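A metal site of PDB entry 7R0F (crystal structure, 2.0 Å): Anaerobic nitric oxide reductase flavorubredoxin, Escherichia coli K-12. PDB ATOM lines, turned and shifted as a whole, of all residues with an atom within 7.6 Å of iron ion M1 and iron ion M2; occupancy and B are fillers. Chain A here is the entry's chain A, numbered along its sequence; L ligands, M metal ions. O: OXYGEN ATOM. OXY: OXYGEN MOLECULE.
A ring nitrogen (NE2) of His 23 sits at hydrogen-bond distance from an oxygen (O2) of OXY L2 (3.4 Å). The side-chain hydroxyl of Tyr 194 is in hydrogen-bond range of an oxygen (O1) of OXY L2 (2.8 Å). O2 of OXY L2 lies close to NE2 of His 147 (3.4 Å).
NE2 of His 84 lies close to OG of Ser 226, 3.4 Å away. The backbone NH (N) of His 147 is in hydrogen-bond range of the side-chain hydroxyl (OG) of Ser 151. A ring nitrogen (NE2) of His 23 is in hydrogen-bond range of the side-chain carboxylate of Glu 81. OG of Ser 33 sits at hydrogen-bond distance from ND1 of His 227, at 3.4 Å. OD1 of Asp 150 lies within hydrogen-bond range of ND1 of His 79 (2.9 Å). The backbone carbonyl oxygen (O) of Ser 34 sits at hydrogen-bond distance from a ring nitrogen (ND1) of His 227 (2.7 Å). ND1 of His 79 sits at hydrogen-bond distance from OG of Ser 151, at 3.4 Å. N of Asp 166 sits at hydrogen-bond distance from OG of Ser 226, at 3.2 Å.
Iron ion M1 is bound by an oxygen (O) of O L1 (1.9 Å), a ring nitrogen (NE2) of His 84 (2.1 Å), the side-chain carboxylate (OD1) of Asp 166 (2.3 Å), a ring nitrogen (NE2) of His 227 (2.4 Å) and the side-chain carboxylate (OD2) of Asp 83 (2.4 Å). Iron ion M1 has five donor atoms within binding distance.
O of O L1 is bound to iron ion M2 (1.9 Å). Iron ion M2 is bound by the side-chain carboxylate (OE1) of Glu 81 (2.0 Å). OD2 of Asp 166 is bound to iron ion M2, at 2.1 Å. NE2 of His 147 binds iron ion M2, 2.2 Å away. A ring nitrogen (NE2) of His 79 is bound to iron ion M2, at 2.5 Å. Slightly farther from iron ion M2 lies O2 of OXY L2 (2.8 Å).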
ATOM      1  N   PHE A  22     -22.171  -2.494 -33.440  1.00  0.00           N
ATOM      2  CA  PHE A  22     -21.718  -3.200 -32.246  1.00  0.00           C
ATOM      3  C   PHE A  22     -22.920  -3.638 -31.413  1.00  0.00           C
ATOM      4  O   PHE A  22     -23.976  -2.996 -31.449  1.00  0.00           O
ATOM      5  CB  PHE A  22     -20.788  -2.322 -31.406  1.00  0.00           C
ATOM      6  CG  PHE A  22     -19.336  -2.626 -31.589  1.00  0.00           C
ATOM      7  CD1 PHE A  22     -18.647  -2.164 -32.698  1.00  0.00           C
ATOM      8  CD2 PHE A  22     -18.648  -3.383 -30.644  1.00  0.00           C
ATOM      9  CE1 PHE A  22     -17.302  -2.457 -32.868  1.00  0.00           C
ATOM     10  CE2 PHE A  22     -17.306  -3.667 -30.814  1.00  0.00           C
ATOM     11  CZ  PHE A  22     -16.641  -3.201 -31.924  1.00  0.00           C
ATOM     12  N   HIS A  23     -22.763  -4.743 -30.682  1.00  0.00           N
ATOM     13  CA  HIS A  23     -23.825  -5.307 -29.865  1.00  0.00           C
ATOM     14  C   HIS A  23     -25.087  -5.521 -30.698  1.00  0.00           C
ATOM     15  O   HIS A  23     -26.173  -5.052 -30.343  1.00  0.00           O
ATOM     16  CB  HIS A  23     -24.132  -4.400 -28.670  1.00  0.00           C
ATOM     17  CG  HIS A  23     -22.959  -4.161 -27.777  1.00  0.00           C
ATOM     18  ND1 HIS A  23     -22.784  -2.979 -27.077  1.00  0.00           N
ATOM     19  CD2 HIS A  23     -21.894  -4.942 -27.473  1.00  0.00           C
ATOM     20  CE1 HIS A  23     -21.658  -3.052 -26.381  1.00  0.00           C
ATOM     21  NE2 HIS A  23     -21.104  -4.230 -26.601  1.00  0.00           N
ATOM     22  N   SER A  33     -13.776   1.564 -35.329  1.00  0.00           N
ATOM     23  CA  SER A  33     -13.198   1.288 -34.024  1.00  0.00           C
ATOM     24  C   SER A  33     -11.862   0.585 -34.169  1.00  0.00           C
ATOM     25  O   SER A  33     -11.392   0.338 -35.282  1.00  0.00           O
ATOM     26  CB  SER A  33     -14.141   0.434 -33.170  1.00  0.00           C
ATOM     27  OG  SER A  33     -13.581   0.164 -31.896  1.00  0.00           O
ATOM     28  N   SER A  34     -11.234   0.286 -33.036  1.00  0.00           N
ATOM     29  CA  SER A  34     -10.021  -0.508 -33.033  1.00  0.00           C
ATOM     30  C   SER A  34     -10.070  -1.514 -31.902  1.00  0.00           C
ATOM     31  O   SER A  34     -10.768  -1.310 -30.909  1.00  0.00           O
ATOM     32  CB  SER A  34      -8.782   0.390 -32.898  1.00  0.00           C
ATOM     33  OG  SER A  34      -8.721   0.986 -31.615  1.00  0.00           O
ATOM     34  N   TYR A  35      -9.346  -2.613 -32.061  1.00  0.00           N
ATOM     35  CA  TYR A  35      -9.249  -3.606 -31.020  1.00  0.00           C
ATOM     36  C   TYR A  35      -7.796  -3.703 -30.600  1.00  0.00           C
ATOM     37  O   TYR A  35      -6.980  -4.295 -31.309  1.00  0.00           O
ATOM     38  CB  TYR A  35      -9.791  -4.951 -31.512  1.00  0.00           C
ATOM     39  CG  TYR A  35     -11.054  -4.801 -32.314  1.00  0.00           C
ATOM     40  CD1 TYR A  35     -12.256  -4.464 -31.701  1.00  0.00           C
ATOM     41  CD2 TYR A  35     -11.044  -4.978 -33.691  1.00  0.00           C
ATOM     42  CE1 TYR A  35     -13.415  -4.317 -32.436  1.00  0.00           C
ATOM     43  CE2 TYR A  35     -12.206  -4.831 -34.440  1.00  0.00           C
ATOM     44  CZ  TYR A  35     -13.386  -4.499 -33.803  1.00  0.00           C
ATOM     45  OH  TYR A  35     -14.536  -4.349 -34.533  1.00  0.00           O
ATOM     46  N   HIS A  79     -10.901  -8.882 -20.026  1.00  0.00           N
ATOM     47  CA  HIS A  79     -12.319  -8.839 -20.379  1.00  0.00           C
ATOM     48  C   HIS A  79     -12.562  -9.823 -21.519  1.00  0.00           C
ATOM     49  O   HIS A  79     -11.859  -9.797 -22.526  1.00  0.00           O
ATOM     50  CB  HIS A  79     -12.694  -7.408 -20.777  1.00  0.00           C
ATOM     51  CG  HIS A  79     -14.142  -7.228 -21.123  1.00  0.00           C
ATOM     52  ND1 HIS A  79     -15.166  -7.739 -20.355  1.00  0.00           N
ATOM     53  CD2 HIS A  79     -14.733  -6.566 -22.147  1.00  0.00           C
ATOM     54  CE1 HIS A  79     -16.316  -7.416 -20.904  1.00  0.00           C
ATOM     55  NE2 HIS A  79     -16.084  -6.701 -21.987  1.00  0.00           N
ATOM     56  N   ALA A  80     -13.560 -10.679 -21.354  1.00  0.00           N
ATOM     57  CA  ALA A  80     -13.749 -11.798 -22.281  1.00  0.00           C
ATOM     58  C   ALA A  80     -14.876 -11.573 -23.285  1.00  0.00           C
ATOM     59  O   ALA A  80     -15.433 -12.536 -23.809  1.00  0.00           O
ATOM     60  CB  ALA A  80     -13.994 -13.082 -21.514  1.00  0.00           C
ATOM     61  N   GLU A  81     -15.203 -10.319 -23.562  1.00  0.00           N
ATOM     62  CA  GLU A  81     -16.156 -10.021 -24.631  1.00  0.00           C
ATOM     63  C   GLU A  81     -15.483 -10.340 -25.970  1.00  0.00           C
ATOM     64  O   GLU A  81     -14.263 -10.265 -26.084  1.00  0.00           O
ATOM     65  CB  GLU A  81     -16.623  -8.565 -24.567  1.00  0.00           C
ATOM     66  CG  GLU A  81     -17.827  -8.260 -25.460  1.00  0.00           C
ATOM     67  CD  GLU A  81     -18.530  -6.972 -25.083  1.00  0.00           C
ATOM     68  OE1 GLU A  81     -18.092  -6.303 -24.123  1.00  0.00           O
ATOM     69  OE2 GLU A  81     -19.533  -6.635 -25.745  1.00  0.00           O
ATOM     70  N   GLU A  82     -16.292 -10.690 -26.960  1.00  0.00           N
ATOM     71  CA  GLU A  82     -15.791 -11.216 -28.234  1.00  0.00           C
ATOM     72  C   GLU A  82     -14.800 -10.299 -28.958  1.00  0.00           C
ATOM     73  O   GLU A  82     -14.003 -10.770 -29.772  1.00  0.00           O
ATOM     74  CB  GLU A  82     -16.965 -11.506 -29.183  1.00  0.00           C
ATOM     75  CG  GLU A  82     -17.662 -10.271 -29.712  1.00  0.00           C
ATOM     76  CD  GLU A  82     -18.795 -10.601 -30.669  1.00  0.00           C
ATOM     77  OE1 GLU A  82     -19.021 -11.796 -30.937  1.00  0.00           O
ATOM     78  OE2 GLU A  82     -19.462  -9.660 -31.153  1.00  0.00           O
ATOM     79  N   ASP A  83     -14.842  -9.005 -28.668  1.00  0.00           N
ATOM     80  CA  ASP A  83     -13.983  -8.065 -29.380  1.00  0.00           C
ATOM     81  C   ASP A  83     -12.604  -7.938 -28.740  1.00  0.00           C
ATOM     82  O   ASP A  83     -11.758  -7.173 -29.190  1.00  0.00           O
ATOM     83  CB  ASP A  83     -14.653  -6.685 -29.441  1.00  0.00           C
ATOM     84  CG  ASP A  83     -15.019  -6.142 -28.079  1.00  0.00           C
ATOM     85  OD1 ASP A  83     -15.235  -6.963 -27.155  1.00  0.00           O
ATOM     86  OD2 ASP A  83     -15.088  -4.905 -27.918  1.00  0.00           O
ATOM     87  N   HIS A  84     -12.374  -8.716 -27.681  1.00  0.00           N
ATOM     88  CA  HIS A  84     -11.075  -8.706 -27.014  1.00  0.00           C
ATOM     89  C   HIS A  84     -10.550 -10.131 -26.809  1.00  0.00           C
ATOM     90  O   HIS A  84      -9.340 -10.343 -26.750  1.00  0.00           O
ATOM     91  CB  HIS A  84     -11.158  -7.977 -25.670  1.00  0.00           C
ATOM     92  CG  HIS A  84     -11.847  -6.655 -25.753  1.00  0.00           C
ATOM     93  ND1 HIS A  84     -11.415  -5.647 -26.605  1.00  0.00           N
ATOM     94  CD2 HIS A  84     -12.929  -6.159 -25.114  1.00  0.00           C
ATOM     95  CE1 HIS A  84     -12.214  -4.601 -26.474  1.00  0.00           C
ATOM     96  NE2 HIS A  84     -13.130  -4.885 -25.572  1.00  0.00           N
ATOM     97  N   LEU A 146     -17.938  -3.288 -14.577  1.00  0.00           N
ATOM     98  CA  LEU A 146     -17.432  -2.146 -15.353  1.00  0.00           C
ATOM     99  C   LEU A 146     -16.695  -2.625 -16.605  1.00  0.00           C
ATOM    100  O   LEU A 146     -15.474  -2.540 -16.683  1.00  0.00           O
ATOM    101  CB  LEU A 146     -16.505  -1.290 -14.496  1.00  0.00           C
ATOM    102  CG  LEU A 146     -17.132  -0.570 -13.302  1.00  0.00           C
ATOM    103  CD1 LEU A 146     -16.068   0.086 -12.441  1.00  0.00           C
ATOM    104  CD2 LEU A 146     -18.157   0.465 -13.770  1.00  0.00           C
ATOM    105  N   HIS A 147     -17.446  -3.124 -17.602  1.00  0.00           N
ATOM    106  CA  HIS A 147     -18.903  -3.142 -17.560  1.00  0.00           C
ATOM    107  C   HIS A 147     -19.447  -4.562 -17.432  1.00  0.00           C
ATOM    108  O   HIS A 147     -20.664  -4.779 -17.479  1.00  0.00           O
ATOM    109  CB  HIS A 147     -19.477  -2.470 -18.816  1.00  0.00           C
ATOM    110  CG  HIS A 147     -19.145  -3.192 -20.079  1.00  0.00           C
ATOM    111  ND1 HIS A 147     -20.008  -4.096 -20.679  1.00  0.00           N
ATOM    112  CD2 HIS A 147     -18.045  -3.148 -20.877  1.00  0.00           C
ATOM    113  CE1 HIS A 147     -19.450  -4.568 -21.774  1.00  0.00           C
ATOM    114  NE2 HIS A 147     -18.264  -4.013 -21.914  1.00  0.00           N
ATOM    115  N   TRP A 148     -18.550  -5.524 -17.263  1.00  0.00           N
ATOM    116  CA  TRP A 148     -18.940  -6.922 -17.082  1.00  0.00           C
ATOM    117  C   TRP A 148     -18.424  -7.445 -15.739  1.00  0.00           C
ATOM    118  O   TRP A 148     -17.509  -6.859 -15.156  1.00  0.00           O
ATOM    119  CB  TRP A 148     -18.391  -7.791 -18.218  1.00  0.00           C
ATOM    120  CG  TRP A 148     -19.297  -7.905 -19.415  1.00  0.00           C
ATOM    121  CD1 TRP A 148     -20.344  -7.088 -19.727  1.00  0.00           C
ATOM    122  CD2 TRP A 148     -19.232  -8.896 -20.446  1.00  0.00           C
ATOM    123  NE1 TRP A 148     -20.936  -7.506 -20.887  1.00  0.00           N
ATOM    124  CE2 TRP A 148     -20.274  -8.617 -21.359  1.00  0.00           C
ATOM    125  CE3 TRP A 148     -18.397  -9.992 -20.693  1.00  0.00           C
ATOM    126  CZ2 TRP A 148     -20.495  -9.387 -22.495  1.00  0.00           C
ATOM    127  CZ3 TRP A 148     -18.617 -10.751 -21.816  1.00  0.00           C
ATOM    128  CH2 TRP A 148     -19.665 -10.454 -22.705  1.00  0.00           C
ATOM    129  N   ASP A 150     -16.602  -9.914 -15.334  1.00  0.00           N
ATOM    130  CA  ASP A 150     -15.251 -10.434 -15.530  1.00  0.00           C
ATOM    131  C   ASP A 150     -14.210  -9.337 -15.698  1.00  0.00           C
ATOM    132  O   ASP A 150     -13.012  -9.614 -15.750  1.00  0.00           O
ATOM    133  CB  ASP A 150     -15.223 -11.370 -16.745  1.00  0.00           C
ATOM    134  CG  ASP A 150     -15.404 -10.625 -18.072  1.00  0.00           C
ATOM    135  OD1 ASP A 150     -15.788  -9.445 -18.059  1.00  0.00           O
ATOM    136  OD2 ASP A 150     -15.153 -11.238 -19.129  1.00  0.00           O
ATOM    137  N   SER A 151     -14.671  -8.095 -15.785  1.00  0.00           N
ATOM    138  CA  SER A 151     -13.812  -6.974 -16.141  1.00  0.00           C
ATOM    139  C   SER A 151     -12.733  -6.682 -15.095  1.00  0.00           C
ATOM    140  O   SER A 151     -12.998  -6.732 -13.887  1.00  0.00           O
ATOM    141  CB  SER A 151     -14.648  -5.722 -16.386  1.00  0.00           C
ATOM    142  OG  SER A 151     -15.540  -5.907 -17.473  1.00  0.00           O
ATOM    143  N   ASN A 165      -8.488  -1.673 -20.562  1.00  0.00           N
ATOM    144  CA  ASN A 165      -9.421  -2.373 -21.441  1.00  0.00           C
ATOM    145  C   ASN A 165     -10.532  -1.425 -21.948  1.00  0.00           C
ATOM    146  O   ASN A 165     -10.236  -0.410 -22.574  1.00  0.00           O
ATOM    147  CB  ASN A 165     -10.028  -3.584 -20.744  1.00  0.00           C
ATOM    148  CG  ASN A 165     -10.659  -4.570 -21.716  1.00  0.00           C
ATOM    149  OD1 ASN A 165     -11.870  -4.563 -21.917  1.00  0.00           O
ATOM    150  ND2 ASN A 165      -9.826  -5.420 -22.313  1.00  0.00           N
ATOM    151  N   ASP A 166     -11.786  -1.774 -21.671  1.00  0.00           N
ATOM    152  CA  ASP A 166     -12.928  -0.981 -22.153  1.00  0.00           C
ATOM    153  C   ASP A 166     -12.991   0.415 -21.534  1.00  0.00           C
ATOM    154  O   ASP A 166     -13.391   1.375 -22.192  1.00  0.00           O
ATOM    155  CB  ASP A 166     -14.242  -1.722 -21.874  1.00  0.00           C
ATOM    156  CG  ASP A 166     -14.617  -2.672 -22.989  1.00  0.00           C
ATOM    157  OD1 ASP A 166     -14.026  -2.583 -24.080  1.00  0.00           O
ATOM    158  OD2 ASP A 166     -15.527  -3.503 -22.782  1.00  0.00           O
ATOM    159  N   ALA A 167     -12.616   0.508 -20.261  1.00  0.00           N
ATOM    160  CA  ALA A 167     -12.681   1.776 -19.539  1.00  0.00           C
ATOM    161  C   ALA A 167     -11.834   2.858 -20.197  1.00  0.00           C
ATOM    162  O   ALA A 167     -10.721   2.587 -20.651  1.00  0.00           O
ATOM    163  CB  ALA A 167     -12.255   1.579 -18.095  1.00  0.00           C
ATOM    164  N   HIS A 171     -14.875   4.114 -29.484  1.00  0.00           N
ATOM    165  CA  HIS A 171     -14.863   3.551 -30.825  1.00  0.00           C
ATOM    166  C   HIS A 171     -14.480   4.631 -31.829  1.00  0.00           C
ATOM    167  O   HIS A 171     -15.334   5.331 -32.368  1.00  0.00           O
ATOM    168  CB  HIS A 171     -16.226   2.933 -31.163  1.00  0.00           C
ATOM    169  CG  HIS A 171     -16.594   1.778 -30.290  1.00  0.00           C
ATOM    170  ND1 HIS A 171     -15.847   0.619 -30.239  1.00  0.00           N
ATOM    171  CD2 HIS A 171     -17.620   1.598 -29.430  1.00  0.00           C
ATOM    172  CE1 HIS A 171     -16.397  -0.225 -29.387  1.00  0.00           C
ATOM    173  NE2 HIS A 171     -17.479   0.347 -28.885  1.00  0.00           N
ATOM    174  N   TYR A 194     -19.602   6.766 -26.091  1.00  0.00           N
ATOM    175  CA  TYR A 194     -19.342   5.454 -25.515  1.00  0.00           C
ATOM    176  C   TYR A 194     -19.876   5.354 -24.094  1.00  0.00           C
ATOM    177  O   TYR A 194     -20.597   4.409 -23.770  1.00  0.00           O
ATOM    178  CB  TYR A 194     -17.845   5.150 -25.535  1.00  0.00           C
ATOM    179  CG  TYR A 194     -17.511   3.757 -25.025  1.00  0.00           C
ATOM    180  CD1 TYR A 194     -17.614   2.662 -25.866  1.00  0.00           C
ATOM    181  CD2 TYR A 194     -17.100   3.558 -23.716  1.00  0.00           C
ATOM    182  CE1 TYR A 194     -17.311   1.386 -25.398  1.00  0.00           C
ATOM    183  CE2 TYR A 194     -16.800   2.292 -23.248  1.00  0.00           C
ATOM    184  CZ  TYR A 194     -16.912   1.215 -24.103  1.00  0.00           C
ATOM    185  OH  TYR A 194     -16.608  -0.050 -23.643  1.00  0.00           O
ATOM    186  N   ILE A 198     -23.147   3.005 -22.878  1.00  0.00           N
ATOM    187  CA  ILE A 198     -22.647   1.753 -22.310  1.00  0.00           C
ATOM    188  C   ILE A 198     -22.476   1.792 -20.790  1.00  0.00           C
ATOM    189  O   ILE A 198     -22.910   0.871 -20.096  1.00  0.00           O
ATOM    190  CB  ILE A 198     -21.298   1.366 -22.945  1.00  0.00           C
ATOM    191  CG1 ILE A 198     -21.420   1.268 -24.460  1.00  0.00           C
ATOM    192  CG2 ILE A 198     -20.791   0.054 -22.361  1.00  0.00           C
ATOM    193  CD1 ILE A 198     -22.455   0.269 -24.929  1.00  0.00           C
ATOM    194  N   SER A 226      -8.607  -0.717 -24.657  1.00  0.00           N
ATOM    195  CA  SER A 226      -8.801  -1.774 -25.645  1.00  0.00           C
ATOM    196  C   SER A 226      -9.486  -1.239 -26.893  1.00  0.00           C
ATOM    197  O   SER A 226      -9.623  -1.956 -27.894  1.00  0.00           O
ATOM    198  CB  SER A 226      -9.622  -2.920 -25.042  1.00  0.00           C
ATOM    199  OG  SER A 226     -10.928  -2.483 -24.721  1.00  0.00           O
ATOM    200  N   HIS A 227      -9.927   0.017 -26.840  1.00  0.00           N
ATOM    201  CA  HIS A 227     -10.591   0.639 -27.981  1.00  0.00           C
ATOM    202  C   HIS A 227     -10.096   2.068 -28.192  1.00  0.00           C
ATOM    203  O   HIS A 227     -10.097   2.893 -27.272  1.00  0.00           O
ATOM    204  CB  HIS A 227     -12.108   0.654 -27.794  1.00  0.00           C
ATOM    205  CG  HIS A 227     -12.744  -0.695 -27.887  1.00  0.00           C
ATOM    206  ND1 HIS A 227     -12.757  -1.436 -29.043  1.00  0.00           N
ATOM    207  CD2 HIS A 227     -13.402  -1.436 -26.961  1.00  0.00           C
ATOM    208  CE1 HIS A 227     -13.401  -2.575 -28.838  1.00  0.00           C
ATOM    209  NE2 HIS A 227     -13.797  -2.601 -27.582  1.00  0.00           N
HETATM  210  O     O L   1     -16.038  -5.020 -25.111  1.00  0.00           O
HETATM  211  O1  OXY L   2     -17.334  -2.283 -25.076  1.00  0.00           O
HETATM  212  O2  OXY L   2     -18.200  -3.104 -25.190  1.00  0.00           O
HETATM  213 FE    FE M   1     -14.844  -3.784 -25.840  1.00  0.00          FE
HETATM  214 FE    FE M   2     -16.889  -4.895 -23.443  1.00  0.00          FE
